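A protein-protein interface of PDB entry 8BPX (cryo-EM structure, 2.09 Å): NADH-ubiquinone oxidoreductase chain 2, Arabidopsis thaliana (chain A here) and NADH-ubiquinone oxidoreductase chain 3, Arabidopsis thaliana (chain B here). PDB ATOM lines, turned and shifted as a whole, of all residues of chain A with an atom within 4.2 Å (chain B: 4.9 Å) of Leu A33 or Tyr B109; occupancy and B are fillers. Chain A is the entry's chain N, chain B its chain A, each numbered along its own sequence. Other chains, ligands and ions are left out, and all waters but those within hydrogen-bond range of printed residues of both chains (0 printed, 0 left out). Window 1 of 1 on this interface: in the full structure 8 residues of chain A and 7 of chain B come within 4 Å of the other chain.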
ATOM      1  N   THR A  29       8.720   0.658  36.254  1.00  0.00           N
ATOM      2  CA  THR A  29       9.633   0.360  35.157  1.00  0.00           C
ATOM      3  C   THR A  29       9.067   0.842  33.828  1.00  0.00           C
ATOM      4  O   THR A  29       9.796   1.401  32.999  1.00  0.00           O
ATOM      5  CB  THR A  29       9.918  -1.142  35.121  1.00  0.00           C
ATOM      6  OG1 THR A  29      10.508  -1.542  36.366  1.00  0.00           O
ATOM      7  CG2 THR A  29      10.862  -1.488  33.987  1.00  0.00           C
ATOM      8  N   PHE A  30       7.767   0.643  33.611  1.00  0.00           N
ATOM      9  CA  PHE A  30       7.143   1.152  32.390  1.00  0.00           C
ATOM     10  C   PHE A  30       7.216   2.674  32.328  1.00  0.00           C
ATOM     11  O   PHE A  30       7.513   3.254  31.273  1.00  0.00           O
ATOM     12  CB  PHE A  30       5.691   0.683  32.311  1.00  0.00           C
ATOM     13  CG  PHE A  30       5.541  -0.799  32.107  1.00  0.00           C
ATOM     14  CD1 PHE A  30       6.620  -1.577  31.722  1.00  0.00           C
ATOM     15  CD2 PHE A  30       4.317  -1.415  32.311  1.00  0.00           C
ATOM     16  CE1 PHE A  30       6.481  -2.943  31.543  1.00  0.00           C
ATOM     17  CE2 PHE A  30       4.174  -2.780  32.130  1.00  0.00           C
ATOM     18  CZ  PHE A  30       5.257  -3.542  31.745  1.00  0.00           C
ATOM     19  N   ILE A  31       6.949   3.334  33.458  1.00  0.00           N
ATOM     20  CA  ILE A  31       7.010   4.792  33.509  1.00  0.00           C
ATOM     21  C   ILE A  31       8.408   5.277  33.151  1.00  0.00           C
ATOM     22  O   ILE A  31       8.571   6.225  32.374  1.00  0.00           O
ATOM     23  CB  ILE A  31       6.572   5.296  34.897  1.00  0.00           C
ATOM     24  CG1 ILE A  31       5.060   5.141  35.067  1.00  0.00           C
ATOM     25  CG2 ILE A  31       6.996   6.747  35.114  1.00  0.00           C
ATOM     26  CD1 ILE A  31       4.584   5.300  36.485  1.00  0.00           C
ATOM     27  N   LEU A  32       9.435   4.633  33.708  1.00  0.00           N
ATOM     28  CA  LEU A  32      10.808   5.038  33.417  1.00  0.00           C
ATOM     29  C   LEU A  32      11.179   4.768  31.966  1.00  0.00           C
ATOM     30  O   LEU A  32      11.891   5.565  31.351  1.00  0.00           O
ATOM     31  CB  LEU A  32      11.782   4.344  34.367  1.00  0.00           C
ATOM     32  CG  LEU A  32      11.543   4.698  35.836  1.00  0.00           C
ATOM     33  CD1 LEU A  32      12.374   3.827  36.772  1.00  0.00           C
ATOM     34  CD2 LEU A  32      11.823   6.171  36.045  1.00  0.00           C
ATOM     35  N   LEU A  33      10.714   3.652  31.400  1.00  0.00           N
ATOM     36  CA  LEU A  33      10.961   3.393  29.984  1.00  0.00           C
ATOM     37  C   LEU A  33      10.401   4.519  29.123  1.00  0.00           C
ATOM     38  O   LEU A  33      11.088   5.043  28.235  1.00  0.00           O
ATOM     39  CB  LEU A  33      10.344   2.054  29.576  1.00  0.00           C
ATOM     40  CG  LEU A  33      10.590   1.613  28.129  1.00  0.00           C
ATOM     41  CD1 LEU A  33      12.078   1.556  27.823  1.00  0.00           C
ATOM     42  CD2 LEU A  33       9.923   0.277  27.832  1.00  0.00           C
ATOM     43  N   ILE A  34       9.156   4.919  29.393  1.00  0.00           N
ATOM     44  CA  ILE A  34       8.525   5.970  28.600  1.00  0.00           C
ATOM     45  C   ILE A  34       9.253   7.299  28.789  1.00  0.00           C
ATOM     46  O   ILE A  34       9.553   8.001  27.817  1.00  0.00           O
ATOM     47  CB  ILE A  34       7.031   6.087  28.953  1.00  0.00           C
ATOM     48  CG1 ILE A  34       6.298   4.793  28.595  1.00  0.00           C
ATOM     49  CG2 ILE A  34       6.404   7.256  28.225  1.00  0.00           C
ATOM     50  CD1 ILE A  34       5.058   4.547  29.413  1.00  0.00           C
ATOM     51  N   HIS A  35       9.538   7.664  30.042  1.00  0.00           N
ATOM     52  CA  HIS A  35      10.275   8.893  30.340  1.00  0.00           C
ATOM     53  C   HIS A  35      11.602   8.938  29.587  1.00  0.00           C
ATOM     54  O   HIS A  35      11.918   9.920  28.896  1.00  0.00           O
ATOM     55  CB  HIS A  35      10.491   8.976  31.857  1.00  0.00           C
ATOM     56  CG  HIS A  35      11.458  10.034  32.293  1.00  0.00           C
ATOM     57  ND1 HIS A  35      11.068  11.322  32.587  1.00  0.00           N
ATOM     58  CD2 HIS A  35      12.791   9.984  32.522  1.00  0.00           C
ATOM     59  CE1 HIS A  35      12.121  12.026  32.959  1.00  0.00           C
ATOM     60  NE2 HIS A  35      13.180  11.237  32.932  1.00  0.00           N
ATOM     61  N   GLY A  36      12.379   7.857  29.694  1.00  0.00           N
ATOM     62  CA  GLY A  36      13.677   7.811  29.051  1.00  0.00           C
ATOM     63  C   GLY A  36      13.585   7.937  27.545  1.00  0.00           C
ATOM     64  O   GLY A  36      14.326   8.706  26.934  1.00  0.00           O
ATOM     65  N   VAL A  37      12.667   7.191  26.923  1.00  0.00           N
ATOM     66  CA  VAL A  37      12.608   7.232  25.466  1.00  0.00           C
ATOM     67  C   VAL A  37      12.068   8.573  24.975  1.00  0.00           C
ATOM     68  O   VAL A  37      12.467   9.047  23.905  1.00  0.00           O
ATOM     69  CB  VAL A  37      11.798   6.048  24.903  1.00  0.00           C
ATOM     70  CG1 VAL A  37      10.300   6.321  24.945  1.00  0.00           C
ATOM     71  CG2 VAL A  37      12.252   5.746  23.486  1.00  0.00           C
ATOM     72  N   PHE A 123      19.938   4.597  29.144  1.00  0.00           N
ATOM     73  CA  PHE A 123      19.030   4.383  30.265  1.00  0.00           C
ATOM     74  C   PHE A 123      18.378   3.007  30.220  1.00  0.00           C
ATOM     75  O   PHE A 123      17.883   2.535  31.248  1.00  0.00           O
ATOM     76  CB  PHE A 123      17.943   5.459  30.287  1.00  0.00           C
ATOM     77  CG  PHE A 123      16.889   5.271  29.236  1.00  0.00           C
ATOM     78  CD1 PHE A 123      15.749   4.524  29.496  1.00  0.00           C
ATOM     79  CD2 PHE A 123      17.039   5.838  27.983  1.00  0.00           C
ATOM     80  CE1 PHE A 123      14.785   4.346  28.528  1.00  0.00           C
ATOM     81  CE2 PHE A 123      16.078   5.663  27.011  1.00  0.00           C
ATOM     82  CZ  PHE A 123      14.952   4.916  27.280  1.00  0.00           C
ATOM     83  N   GLU A 124      18.345   2.370  29.047  1.00  0.00           N
ATOM     84  CA  GLU A 124      17.737   1.048  28.928  1.00  0.00           C
ATOM     85  C   GLU A 124      18.430   0.034  29.826  1.00  0.00           C
ATOM     86  O   GLU A 124      17.829  -0.974  30.204  1.00  0.00           O
ATOM     87  CB  GLU A 124      17.772   0.587  27.471  1.00  0.00           C
ATOM     88  CG  GLU A 124      16.836   1.363  26.550  1.00  0.00           C
ATOM     89  CD  GLU A 124      17.498   2.574  25.902  1.00  0.00           C
ATOM     90  OE1 GLU A 124      18.466   3.115  26.474  1.00  0.00           O
ATOM     91  OE2 GLU A 124      17.040   2.988  24.819  1.00  0.00           O
ATOM     92  N   ILE B 105       3.539  -0.750  24.883  1.00  0.00           N
ATOM     93  CA  ILE B 105       4.641   0.058  25.402  1.00  0.00           C
ATOM     94  C   ILE B 105       5.920  -0.265  24.644  1.00  0.00           C
ATOM     95  O   ILE B 105       6.683   0.635  24.261  1.00  0.00           O
ATOM     96  CB  ILE B 105       4.806  -0.153  26.916  1.00  0.00           C
ATOM     97  CG1 ILE B 105       3.708   0.588  27.673  1.00  0.00           C
ATOM     98  CG2 ILE B 105       6.183   0.311  27.380  1.00  0.00           C
ATOM     99  CD1 ILE B 105       3.847   0.486  29.160  1.00  0.00           C
ATOM    100  N   GLY B 106       6.171  -1.554  24.408  1.00  0.00           N
ATOM    101  CA  GLY B 106       7.296  -1.921  23.559  1.00  0.00           C
ATOM    102  C   GLY B 106       7.209  -1.308  22.169  1.00  0.00           C
ATOM    103  O   GLY B 106       8.210  -0.832  21.621  1.00  0.00           O
ATOM    104  N   PHE B 107       6.014  -1.317  21.583  1.00  0.00           N
ATOM    105  CA  PHE B 107       5.821  -0.726  20.262  1.00  0.00           C
ATOM    106  C   PHE B 107       6.105   0.773  20.273  1.00  0.00           C
ATOM    107  O   PHE B 107       6.716   1.299  19.340  1.00  0.00           O
ATOM    108  CB  PHE B 107       4.399  -0.993  19.770  1.00  0.00           C
ATOM    109  CG  PHE B 107       4.181  -0.654  18.322  1.00  0.00           C
ATOM    110  CD1 PHE B 107       4.943  -1.251  17.331  1.00  0.00           C
ATOM    111  CD2 PHE B 107       3.214   0.263  17.952  1.00  0.00           C
ATOM    112  CE1 PHE B 107       4.740  -0.939  15.997  1.00  0.00           C
ATOM    113  CE2 PHE B 107       3.008   0.580  16.621  1.00  0.00           C
ATOM    114  CZ  PHE B 107       3.767  -0.022  15.644  1.00  0.00           C
ATOM    115  N   LEU B 108       5.652   1.476  21.313  1.00  0.00           N
ATOM    116  CA  LEU B 108       5.941   2.900  21.439  1.00  0.00           C
ATOM    117  C   LEU B 108       7.440   3.145  21.537  1.00  0.00           C
ATOM    118  O   LEU B 108       7.969   4.080  20.923  1.00  0.00           O
ATOM    119  CB  LEU B 108       5.225   3.481  22.658  1.00  0.00           C
ATOM    120  CG  LEU B 108       5.492   4.950  23.003  1.00  0.00           C
ATOM    121  CD1 LEU B 108       5.204   5.868  21.821  1.00  0.00           C
ATOM    122  CD2 LEU B 108       4.683   5.374  24.221  1.00  0.00           C
ATOM    123  N   TYR B 109       8.138   2.308  22.308  1.00  0.00           N
ATOM    124  CA  TYR B 109       9.593   2.398  22.376  1.00  0.00           C
ATOM    125  C   TYR B 109      10.218   2.245  20.994  1.00  0.00           C
ATOM    126  O   TYR B 109      11.105   3.017  20.613  1.00  0.00           O
ATOM    127  CB  TYR B 109      10.144   1.337  23.328  1.00  0.00           C
ATOM    128  CG  TYR B 109      11.652   1.308  23.382  1.00  0.00           C
ATOM    129  CD1 TYR B 109      12.360   2.260  24.103  1.00  0.00           C
ATOM    130  CD2 TYR B 109      12.369   0.346  22.688  1.00  0.00           C
ATOM    131  CE1 TYR B 109      13.741   2.242  24.145  1.00  0.00           C
ATOM    132  CE2 TYR B 109      13.747   0.318  22.724  1.00  0.00           C
ATOM    133  CZ  TYR B 109      14.429   1.267  23.454  1.00  0.00           C
ATOM    134  OH  TYR B 109      15.801   1.240  23.485  1.00  0.00           O
ATOM    135  N   GLU B 110       9.770   1.248  20.228  1.00  0.00           N
ATOM    136  CA  GLU B 110      10.316   1.061  18.884  1.00  0.00           C
ATOM    137  C   GLU B 110      10.020   2.262  17.994  1.00  0.00           C
ATOM    138  O   GLU B 110      10.881   2.702  17.226  1.00  0.00           O
ATOM    139  CB  GLU B 110       9.760  -0.209  18.243  1.00  0.00           C
ATOM    140  CG  GLU B 110      10.519  -1.469  18.589  1.00  0.00           C
ATOM    141  CD  GLU B 110       9.589  -2.642  18.751  1.00  0.00           C
ATOM    142  OE1 GLU B 110       8.361  -2.413  18.726  1.00  0.00           O
ATOM    143  OE2 GLU B 110      10.075  -3.781  18.905  1.00  0.00           O
ATOM    144  N   TRP B 111       8.802   2.793  18.083  1.00  0.00           N
ATOM    145  CA  TRP B 111       8.400   3.931  17.263  1.00  0.00           C
ATOM    146  C   TRP B 111       9.281   5.143  17.542  1.00  0.00           C
ATOM    147  O   TRP B 111       9.772   5.794  16.615  1.00  0.00           O
ATOM    148  CB  TRP B 111       6.930   4.248  17.544  1.00  0.00           C
ATOM    149  CG  TRP B 111       6.277   5.254  16.656  1.00  0.00           C
ATOM    150  CD1 TRP B 111       6.737   6.496  16.327  1.00  0.00           C
ATOM    151  CD2 TRP B 111       5.008   5.113  16.012  1.00  0.00           C
ATOM    152  NE1 TRP B 111       5.838   7.129  15.507  1.00  0.00           N
ATOM    153  CE2 TRP B 111       4.765   6.304  15.302  1.00  0.00           C
ATOM    154  CE3 TRP B 111       4.055   4.093  15.964  1.00  0.00           C
ATOM    155  CZ2 TRP B 111       3.613   6.498  14.544  1.00  0.00           C
ATOM    156  CZ3 TRP B 111       2.909   4.291  15.219  1.00  0.00           C
ATOM    157  CH2 TRP B 111       2.701   5.481  14.516  1.00  0.00           C
ATOM    158  N   LYS B 112       9.503   5.446  18.823  1.00  0.00           N
ATOM    159  CA  LYS B 112      10.298   6.614  19.190  1.00  0.00           C
ATOM    160  C   LYS B 112      11.748   6.464  18.744  1.00  0.00           C
ATOM    161  O   LYS B 112      12.375   7.435  18.305  1.00  0.00           O
ATOM    162  CB  LYS B 112      10.221   6.837  20.700  1.00  0.00           C
ATOM    163  CG  LYS B 112       8.889   7.371  21.186  1.00  0.00           C
ATOM    164  CD  LYS B 112       8.457   8.597  20.407  1.00  0.00           C
ATOM    165  CE  LYS B 112       9.003   9.866  21.040  1.00  0.00           C
ATOM    166  NZ  LYS B 112       9.504  10.840  20.030  1.00  0.00           N
ATOM    167  N   ARG B 113      12.292   5.253  18.834  1.00  0.00           N
ATOM    168  CA  ARG B 113      13.685   4.994  18.497  1.00  0.00           C
ATOM    169  C   ARG B 113      13.954   4.964  16.997  1.00  0.00           C
ATOM    170  O   ARG B 113      15.115   4.836  16.602  1.00  0.00           O
ATOM    171  CB  ARG B 113      14.139   3.672  19.123  1.00  0.00           C
ATOM    172  CG  ARG B 113      14.476   3.771  20.599  1.00  0.00           C
ATOM    173  CD  ARG B 113      15.920   4.178  20.787  1.00  0.00           C
ATOM    174  NE  ARG B 113      16.266   4.405  22.183  1.00  0.00           N
ATOM    175  CZ  ARG B 113      16.502   5.598  22.711  1.00  0.00           C
ATOM    176  NH1 ARG B 113      16.367   6.706  22.006  1.00  0.00           N
ATOM    177  NH2 ARG B 113      16.899   5.678  23.978  1.00  0.00           N
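OH of Tyr B109 sits at hydrogen-bond distance from OE2 of Glu A124 (2.5 Å). The guanidinium group of Arg B113 lies within salt-bridge range of the side-chain carboxylate of Glu A124 (2.8 Å).
The guanidinium group of Arg B113 is in hydrogen-bond range of the side-chain hydroxyl of Tyr B109, 3.5 Å away.
Ile B105 touches Phe A30. Leu A33 touches Ile B105. CD1 of Leu A33 touches CD1 of Tyr B109, at 3.8 Å. Val A37 touches Tyr B109 (CG2 to CD1, 3.5 Å). Lys B112 touches Val A37 (CB to CG2, 3.6 Å). Phe A123 touches Arg B113.
Leu A33 touches two residues of chain B. Tyr B109 touches just these residues of chain A: Leu A33 (3.8 Å), Val A37 (3.5 Å) and Glu A124 (2.5 Å). Printed residues of chain A within 4 Å of Lys B112: Val A37 (3.6 Å). Of the printed residues of chain B, Phe A30 touches Ile B105 (3.6 Å). The nearest printed residue of chain B that does not touch Leu A33 is Gly B106 (5.4 Å).
Of the 11 printed residues of chain A, 5 touch a printed residue of chain B. Hydrophobic or aromatic side chains of chain A that line the printed part of chain B: Phe A30, Leu A33, Val A37 and Phe A123. Hydrophobic or aromatic side chains of chain B within 4 Å of the printed part of chain A: Ile B105 and Tyr B109.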
